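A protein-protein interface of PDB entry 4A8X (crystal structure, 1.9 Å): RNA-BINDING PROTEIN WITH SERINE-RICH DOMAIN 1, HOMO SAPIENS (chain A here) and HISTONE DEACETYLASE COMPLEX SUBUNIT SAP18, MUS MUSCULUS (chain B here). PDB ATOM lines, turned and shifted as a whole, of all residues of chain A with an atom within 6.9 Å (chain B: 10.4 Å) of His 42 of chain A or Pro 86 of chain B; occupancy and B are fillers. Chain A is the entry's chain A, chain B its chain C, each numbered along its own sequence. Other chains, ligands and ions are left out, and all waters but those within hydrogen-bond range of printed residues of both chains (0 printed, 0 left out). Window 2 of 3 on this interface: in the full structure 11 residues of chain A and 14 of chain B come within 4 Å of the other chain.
A ring nitrogen (NE2) of His 42 of chain A sits close to the side-chain sulfur of Met 81 of chain B (3.8 Å). NE2 of His 44 of chain A lies within hydrogen-bond range of OH of Tyr 88 of chain B.
N of Glu 39 of chain A sits at hydrogen-bond distance from O of Leu 45 of chain A.
Of the printed residues of chain B, Glu 39 of chain A touches Leu 83 (3.7 Å). Met 41 of chain A touches none of the printed residues of chain B. Printed residues of chain B within 4 Å of His 42 of chain A: Met 81, Leu 83 and Pro 86. Of chain B, only Arg 35 (3.7 Å), Gly 36 (3.6 Å) and Tyr 88 (2.7 Å) come within 4 Å of His 44 of chain A. Of the printed residues of chain B, Leu 45 of chain A touches Met 81 (3.7 Å). Of the printed residues of chain A, Gly 36 of chain B touches His 44 (3.6 Å). Of the printed residues of chain A, Met 81 of chain B touches His 42 (3.7 Å) and Leu 45 (3.7 Å). Asp 82 of chain B touches none of the printed residues of chain A. Of the printed residues of chain A, Pro 86 of chain B touches His 42. Tyr 119 of chain B touches none of the printed residues of chain A. The nearest printed residue of chain B that does not touch His 42 of chain A is Gly 87 of chain B (4.1 Å). The nearest printed residue of chain A that does not touch Pro 86 of chain B is Met 41 of chain A (5.5 Å). The nearest printed residue of chain A that does not touch Tyr 88 of chain B is Leu 45 of chain A (4.2 Å).
Hydrophobic or aromatic side chains of chain A that line the printed part of chain B: His 42, His 44 and Leu 45. Hydrophobic or aromatic side chains of chain B within 4 Å of the printed part of chain A: Met 81, Leu 83 and Tyr 88. Among the printed residues, 8 pairs touch across the chains.
Among the printed residues, merely in contact across the chains: Glu 39 of chain A with Leu 83 of chain B, His 42 of chain A with Leu 83 of chain B, His 42 of chain A with Pro 86 of chain B, His 44 of chain A with Arg 35 of chain B, His 44 of chain A with Gly 36 of chain B and Leu 45 of chain A with Met 81 of chain B.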
ATOM      1  N   VAL A  38     -19.029  26.997  36.580  1.00  0.00           N
ATOM      2  CA  VAL A  38     -19.968  26.285  35.718  1.00  0.00           C
ATOM      3  C   VAL A  38     -19.712  26.634  34.265  1.00  0.00           C
ATOM      4  O   VAL A  38     -19.110  27.655  33.971  1.00  0.00           O
ATOM      5  CB  VAL A  38     -21.426  26.686  36.035  1.00  0.00           C
ATOM      6  CG1 VAL A  38     -21.723  26.431  37.489  1.00  0.00           C
ATOM      7  CG2 VAL A  38     -21.678  28.165  35.670  1.00  0.00           C
ATOM      8  N   GLU A  39     -20.193  25.792  33.358  1.00  0.00           N
ATOM      9  CA  GLU A  39     -20.071  26.067  31.929  1.00  0.00           C
ATOM     10  C   GLU A  39     -20.876  27.336  31.573  1.00  0.00           C
ATOM     11  O   GLU A  39     -22.088  27.415  31.823  1.00  0.00           O
ATOM     12  CB  GLU A  39     -20.513  24.852  31.112  1.00  0.00           C
ATOM     13  CG  GLU A  39     -19.563  23.658  31.206  1.00  0.00           C
ATOM     14  CD  GLU A  39     -18.287  23.854  30.391  1.00  0.00           C
ATOM     15  OE1 GLU A  39     -18.197  24.872  29.679  1.00  0.00           O
ATOM     16  OE2 GLU A  39     -17.371  23.001  30.477  1.00  0.00           O
ATOM     17  N   ARG A  40     -20.177  28.332  31.042  1.00  0.00           N
ATOM     18  CA  ARG A  40     -20.795  29.594  30.615  1.00  0.00           C
ATOM     19  C   ARG A  40     -22.098  29.376  29.842  1.00  0.00           C
ATOM     20  O   ARG A  40     -23.159  29.897  30.206  1.00  0.00           O
ATOM     21  CB  ARG A  40     -19.812  30.390  29.750  1.00  0.00           C
ATOM     22  CG  ARG A  40     -18.629  30.947  30.519  1.00  0.00           C
ATOM     23  CD  ARG A  40     -17.689  31.780  29.636  1.00  0.00           C
ATOM     24  NE  ARG A  40     -16.555  32.311  30.404  1.00  0.00           N
ATOM     25  CZ  ARG A  40     -15.613  33.120  29.913  1.00  0.00           C
ATOM     26  NH1 ARG A  40     -15.656  33.499  28.640  1.00  0.00           N
ATOM     27  NH2 ARG A  40     -14.623  33.548  30.697  1.00  0.00           N
ATOM     28  N   MET A  41     -22.011  28.565  28.796  1.00  0.00           N
ATOM     29  CA  MET A  41     -23.133  28.340  27.899  1.00  0.00           C
ATOM     30  C   MET A  41     -24.045  27.193  28.353  1.00  0.00           C
ATOM     31  O   MET A  41     -25.092  26.961  27.742  1.00  0.00           O
ATOM     32  CB  MET A  41     -22.602  28.072  26.488  1.00  0.00           C
ATOM     33  CG  MET A  41     -21.559  29.102  26.001  1.00  0.00           C
ATOM     34  SD  MET A  41     -22.141  30.815  25.757  1.00  0.00           S
ATOM     35  CE  MET A  41     -23.565  30.569  24.675  1.00  0.00           C
ATOM     36  N   HIS A  42     -23.636  26.446  29.382  1.00  0.00           N
ATOM     37  CA  HIS A  42     -24.503  25.447  30.006  1.00  0.00           C
ATOM     38  C   HIS A  42     -24.331  25.477  31.527  1.00  0.00           C
ATOM     39  O   HIS A  42     -23.678  24.599  32.094  1.00  0.00           O
ATOM     40  CB  HIS A  42     -24.162  24.054  29.480  1.00  0.00           C
ATOM     41  CG  HIS A  42     -23.653  24.056  28.073  1.00  0.00           C
ATOM     42  ND1 HIS A  42     -24.474  24.281  26.988  1.00  0.00           N
ATOM     43  CD2 HIS A  42     -22.409  23.873  27.574  1.00  0.00           C
ATOM     44  CE1 HIS A  42     -23.756  24.231  25.880  1.00  0.00           C
ATOM     45  NE2 HIS A  42     -22.501  23.979  26.208  1.00  0.00           N
ATOM     46  N   PRO A  43     -24.921  26.483  32.191  1.00  0.00           N
ATOM     47  CA  PRO A  43     -24.735  26.711  33.635  1.00  0.00           C
ATOM     48  C   PRO A  43     -25.106  25.541  34.556  1.00  0.00           C
ATOM     49  O   PRO A  43     -24.700  25.549  35.713  1.00  0.00           O
ATOM     50  CB  PRO A  43     -25.634  27.931  33.918  1.00  0.00           C
ATOM     51  CG  PRO A  43     -26.606  27.980  32.798  1.00  0.00           C
ATOM     52  CD  PRO A  43     -25.893  27.425  31.602  1.00  0.00           C
ATOM     53  N   HIS A  44     -25.866  24.567  34.073  1.00  0.00           N
ATOM     54  CA  HIS A  44     -26.249  23.450  34.931  1.00  0.00           C
ATOM     55  C   HIS A  44     -25.094  22.453  35.097  1.00  0.00           C
ATOM     56  O   HIS A  44     -25.188  21.507  35.888  1.00  0.00           O
ATOM     57  CB  HIS A  44     -27.519  22.760  34.403  1.00  0.00           C
ATOM     58  CG  HIS A  44     -27.326  21.988  33.131  1.00  0.00           C
ATOM     59  ND1 HIS A  44     -27.333  22.576  31.885  1.00  0.00           N
ATOM     60  CD2 HIS A  44     -27.148  20.663  32.920  1.00  0.00           C
ATOM     61  CE1 HIS A  44     -27.149  21.647  30.959  1.00  0.00           C
ATOM     62  NE2 HIS A  44     -27.030  20.479  31.562  1.00  0.00           N
ATOM     63  N   LEU A  45     -24.018  22.684  34.346  1.00  0.00           N
ATOM     64  CA  LEU A  45     -22.870  21.801  34.311  1.00  0.00           C
ATOM     65  C   LEU A  45     -21.637  22.494  34.869  1.00  0.00           C
ATOM     66  O   LEU A  45     -21.407  23.668  34.618  1.00  0.00           O
ATOM     67  CB  LEU A  45     -22.566  21.366  32.878  1.00  0.00           C
ATOM     68  CG  LEU A  45     -23.678  20.592  32.155  1.00  0.00           C
ATOM     69  CD1 LEU A  45     -23.221  20.241  30.771  1.00  0.00           C
ATOM     70  CD2 LEU A  45     -24.028  19.335  32.932  1.00  0.00           C
ATOM     71  N   SER A  46     -20.829  21.748  35.599  1.00  0.00           N
ATOM     72  CA  SER A  46     -19.570  22.282  36.119  1.00  0.00           C
ATOM     73  C   SER A  46     -18.497  22.173  35.045  1.00  0.00           C
ATOM     74  O   SER A  46     -18.711  21.528  34.011  1.00  0.00           O
ATOM     75  CB  SER A  46     -19.144  21.492  37.371  1.00  0.00           C
ATOM     76  OG  SER A  46     -18.480  20.302  36.971  1.00  0.00           O
ATOM     77  N   MET B  30     -34.111  15.138  22.215  1.00  0.00           N
ATOM     78  CA  MET B  30     -33.061  15.894  22.912  1.00  0.00           C
ATOM     79  C   MET B  30     -33.669  16.999  23.772  1.00  0.00           C
ATOM     80  O   MET B  30     -33.104  17.365  24.807  1.00  0.00           O
ATOM     81  CB  MET B  30     -32.028  16.469  21.926  1.00  0.00           C
ATOM     82  CG  MET B  30     -30.979  15.435  21.431  1.00  0.00           C
ATOM     83  SD  MET B  30     -30.136  14.414  22.719  1.00  0.00           S
ATOM     84  CE  MET B  30     -31.142  12.924  22.831  1.00  0.00           C
ATOM     85  N   ASP B  31     -34.832  17.507  23.360  1.00  0.00           N
ATOM     86  CA  ASP B  31     -35.504  18.555  24.121  1.00  0.00           C
ATOM     87  C   ASP B  31     -35.964  18.073  25.501  1.00  0.00           C
ATOM     88  O   ASP B  31     -36.236  18.891  26.389  1.00  0.00           O
ATOM     89  CB  ASP B  31     -36.685  19.129  23.343  1.00  0.00           C
ATOM     90  CG  ASP B  31     -37.609  18.057  22.839  1.00  0.00           C
ATOM     91  OD1 ASP B  31     -38.275  17.405  23.680  1.00  0.00           O
ATOM     92  OD2 ASP B  31     -37.640  17.859  21.603  1.00  0.00           O
ATOM     93  N   PHE B  33     -33.983  16.748  27.549  1.00  0.00           N
ATOM     94  CA  PHE B  33     -32.755  16.825  28.371  1.00  0.00           C
ATOM     95  C   PHE B  33     -32.202  18.234  28.537  1.00  0.00           C
ATOM     96  O   PHE B  33     -31.218  18.439  29.224  1.00  0.00           O
ATOM     97  CB  PHE B  33     -31.650  15.961  27.776  1.00  0.00           C
ATOM     98  CG  PHE B  33     -31.973  14.504  27.761  1.00  0.00           C
ATOM     99  CD1 PHE B  33     -31.758  13.715  28.891  1.00  0.00           C
ATOM    100  CD2 PHE B  33     -32.511  13.916  26.630  1.00  0.00           C
ATOM    101  CE1 PHE B  33     -32.070  12.353  28.879  1.00  0.00           C
ATOM    102  CE2 PHE B  33     -32.812  12.560  26.613  1.00  0.00           C
ATOM    103  CZ  PHE B  33     -32.601  11.777  27.746  1.00  0.00           C
ATOM    104  N   SER B  34     -32.844  19.211  27.920  1.00  0.00           N
ATOM    105  CA  SER B  34     -32.311  20.563  27.942  1.00  0.00           C
ATOM    106  C   SER B  34     -32.232  21.169  29.337  1.00  0.00           C
ATOM    107  O   SER B  34     -33.183  21.084  30.126  1.00  0.00           O
ATOM    108  CB  SER B  34     -33.162  21.460  27.048  1.00  0.00           C
ATOM    109  OG  SER B  34     -32.997  21.043  25.712  1.00  0.00           O
ATOM    110  N   ARG B  35     -31.096  21.801  29.623  1.00  0.00           N
ATOM    111  CA  ARG B  35     -30.921  22.561  30.869  1.00  0.00           C
ATOM    112  C   ARG B  35     -30.975  21.671  32.118  1.00  0.00           C
ATOM    113  O   ARG B  35     -31.288  22.137  33.224  1.00  0.00           O
ATOM    114  CB  ARG B  35     -31.983  23.659  30.972  1.00  0.00           C
ATOM    115  N   GLY B  36     -30.656  20.393  31.951  1.00  0.00           N
ATOM    116  CA  GLY B  36     -30.508  19.514  33.088  1.00  0.00           C
ATOM    117  C   GLY B  36     -31.802  18.818  33.428  1.00  0.00           C
ATOM    118  O   GLY B  36     -31.812  17.957  34.307  1.00  0.00           O
ATOM    119  N   PHE B  80     -25.169  12.863  25.422  1.00  0.00           N
ATOM    120  CA  PHE B  80     -23.991  13.545  25.926  1.00  0.00           C
ATOM    121  C   PHE B  80     -23.950  14.985  25.512  1.00  0.00           C
ATOM    122  O   PHE B  80     -24.353  15.344  24.396  1.00  0.00           O
ATOM    123  CB  PHE B  80     -22.739  12.844  25.411  1.00  0.00           C
ATOM    124  CG  PHE B  80     -22.604  12.853  23.902  1.00  0.00           C
ATOM    125  CD1 PHE B  80     -23.217  11.876  23.141  1.00  0.00           C
ATOM    126  CD2 PHE B  80     -21.830  13.804  23.265  1.00  0.00           C
ATOM    127  CE1 PHE B  80     -23.082  11.855  21.766  1.00  0.00           C
ATOM    128  CE2 PHE B  80     -21.676  13.792  21.889  1.00  0.00           C
ATOM    129  CZ  PHE B  80     -22.309  12.817  21.136  1.00  0.00           C
ATOM    130  N   MET B  81     -23.455  15.824  26.409  1.00  0.00           N
ATOM    131  CA  MET B  81     -23.337  17.232  26.093  1.00  0.00           C
ATOM    132  C   MET B  81     -22.120  17.392  25.206  1.00  0.00           C
ATOM    133  O   MET B  81     -21.048  16.862  25.486  1.00  0.00           O
ATOM    134  CB  MET B  81     -23.213  18.089  27.365  1.00  0.00           C
ATOM    135  CG  MET B  81     -22.864  19.564  27.105  1.00  0.00           C
ATOM    136  SD  MET B  81     -24.019  20.514  26.047  1.00  0.00           S
ATOM    137  CE  MET B  81     -25.481  20.578  27.091  1.00  0.00           C
ATOM    138  N   ASP B  82     -22.319  18.094  24.109  1.00  0.00           N
ATOM    139  CA  ASP B  82     -21.254  18.414  23.176  1.00  0.00           C
ATOM    140  C   ASP B  82     -21.158  19.915  23.238  1.00  0.00           C
ATOM    141  O   ASP B  82     -22.087  20.603  22.843  1.00  0.00           O
ATOM    142  CB  ASP B  82     -21.618  17.969  21.765  1.00  0.00           C
ATOM    143  CG  ASP B  82     -20.522  18.273  20.754  1.00  0.00           C
ATOM    144  OD1 ASP B  82     -19.674  19.153  21.038  1.00  0.00           O
ATOM    145  OD2 ASP B  82     -20.515  17.637  19.672  1.00  0.00           O
ATOM    146  N   LEU B  83     -20.069  20.420  23.807  1.00  0.00           N
ATOM    147  CA  LEU B  83     -19.900  21.856  23.957  1.00  0.00           C
ATOM    148  C   LEU B  83     -19.788  22.507  22.574  1.00  0.00           C
ATOM    149  O   LEU B  83     -20.208  23.637  22.397  1.00  0.00           O
ATOM    150  CB  LEU B  83     -18.681  22.167  24.854  1.00  0.00           C
ATOM    151  CG  LEU B  83     -18.763  21.585  26.279  1.00  0.00           C
ATOM    152  CD1 LEU B  83     -17.432  21.692  27.060  1.00  0.00           C
ATOM    153  CD2 LEU B  83     -19.891  22.273  27.042  1.00  0.00           C
ATOM    154  N   LYS B  84     -19.271  21.780  21.586  1.00  0.00           N
ATOM    155  CA  LYS B  84     -19.096  22.330  20.228  1.00  0.00           C
ATOM    156  C   LYS B  84     -20.414  22.845  19.589  1.00  0.00           C
ATOM    157  O   LYS B  84     -20.462  23.964  19.063  1.00  0.00           O
ATOM    158  CB  LYS B  84     -18.421  21.297  19.317  1.00  0.00           C
ATOM    159  N   ARG B  85     -21.461  22.017  19.613  1.00  0.00           N
ATOM    160  CA  ARG B  85     -22.832  22.493  19.407  1.00  0.00           C
ATOM    161  C   ARG B  85     -23.344  22.925  20.770  1.00  0.00           C
ATOM    162  O   ARG B  85     -23.032  22.287  21.769  1.00  0.00           O
ATOM    163  CB  ARG B  85     -23.744  21.379  18.881  1.00  0.00           C
ATOM    164  CG  ARG B  85     -25.236  21.760  18.878  1.00  0.00           C
ATOM    165  CD  ARG B  85     -26.142  20.529  18.877  1.00  0.00           C
ATOM    166  NE  ARG B  85     -27.550  20.821  18.561  1.00  0.00           N
ATOM    167  CZ  ARG B  85     -28.022  21.091  17.338  1.00  0.00           C
ATOM    168  NH1 ARG B  85     -27.204  21.141  16.292  1.00  0.00           N
ATOM    169  NH2 ARG B  85     -29.317  21.328  17.158  1.00  0.00           N
ATOM    170  N   PRO B  86     -24.143  23.995  20.835  1.00  0.00           N
ATOM    171  CA  PRO B  86     -24.612  24.310  22.190  1.00  0.00           C
ATOM    172  C   PRO B  86     -25.768  23.404  22.662  1.00  0.00           C
ATOM    173  O   PRO B  86     -26.882  23.901  22.859  1.00  0.00           O
ATOM    174  CB  PRO B  86     -25.043  25.777  22.082  1.00  0.00           C
ATOM    175  CG  PRO B  86     -25.406  25.966  20.630  1.00  0.00           C
ATOM    176  CD  PRO B  86     -24.566  24.991  19.834  1.00  0.00           C
ATOM    177  N   GLY B  87     -25.499  22.108  22.863  1.00  0.00           N
ATOM    178  CA  GLY B  87     -26.529  21.196  23.341  1.00  0.00           C
ATOM    179  C   GLY B  87     -26.236  19.692  23.362  1.00  0.00           C
ATOM    180  O   GLY B  87     -25.198  19.232  22.861  1.00  0.00           O
ATOM    181  N   TYR B  88     -27.173  18.931  23.947  1.00  0.00           N
ATOM    182  CA  TYR B  88     -27.094  17.469  24.011  1.00  0.00           C
ATOM    183  C   TYR B  88     -27.271  16.800  22.661  1.00  0.00           C
ATOM    184  O   TYR B  88     -27.997  17.292  21.800  1.00  0.00           O
ATOM    185  CB  TYR B  88     -28.159  16.916  24.958  1.00  0.00           C
ATOM    186  CG  TYR B  88     -27.889  17.212  26.419  1.00  0.00           C
ATOM    187  CD1 TYR B  88     -26.966  16.465  27.132  1.00  0.00           C
ATOM    188  CD2 TYR B  88     -28.558  18.240  27.079  1.00  0.00           C
ATOM    189  CE1 TYR B  88     -26.705  16.736  28.476  1.00  0.00           C
ATOM    190  CE2 TYR B  88     -28.309  18.510  28.421  1.00  0.00           C
ATOM    191  CZ  TYR B  88     -27.382  17.752  29.106  1.00  0.00           C
ATOM    192  OH  TYR B  88     -27.132  18.018  30.426  1.00  0.00           O
ATOM    193  N   ARG B  89     -26.592  15.674  22.484  1.00  0.00           N
ATOM    194  CA  ARG B  89     -26.678  14.919  21.263  1.00  0.00           C
ATOM    195  C   ARG B  89     -26.868  13.484  21.661  1.00  0.00           C
ATOM    196  O   ARG B  89     -26.589  13.106  22.803  1.00  0.00           O
ATOM    197  CB  ARG B  89     -25.410  15.088  20.430  1.00  0.00           C
ATOM    198  CG  ARG B  89     -25.194  16.526  19.955  1.00  0.00           C
ATOM    199  CD  ARG B  89     -23.944  16.657  19.092  1.00  0.00           C
ATOM    200  NE  ARG B  89     -23.826  15.576  18.122  1.00  0.00           N
ATOM    201  CZ  ARG B  89     -22.674  15.057  17.705  1.00  0.00           C
ATOM    202  NH1 ARG B  89     -21.526  15.520  18.180  1.00  0.00           N
ATOM    203  NH2 ARG B  89     -22.660  14.066  16.822  1.00  0.00           N
ATOM    204  N   TYR B 119     -25.633  10.460  29.830  1.00  0.00           N
ATOM    205  CA  TYR B 119     -26.783   9.568  30.027  1.00  0.00           C
ATOM    206  C   TYR B 119     -26.793   8.336  29.098  1.00  0.00           C
ATOM    207  O   TYR B 119     -26.222   8.365  28.021  1.00  0.00           O
ATOM    208  CB  TYR B 119     -28.072  10.339  29.834  1.00  0.00           C
ATOM    209  CG  TYR B 119     -28.156  11.662  30.548  1.00  0.00           C
ATOM    210  CD1 TYR B 119     -27.904  11.774  31.916  1.00  0.00           C
ATOM    211  CD2 TYR B 119     -28.551  12.795  29.864  1.00  0.00           C
ATOM    212  CE1 TYR B 119     -28.021  12.989  32.564  1.00  0.00           C
ATOM    213  CE2 TYR B 119     -28.675  14.015  30.499  1.00  0.00           C
ATOM    214  CZ  TYR B 119     -28.423  14.110  31.848  1.00  0.00           C
ATOM    215  OH  TYR B 119     -28.560  15.348  32.436  1.00  0.00           O
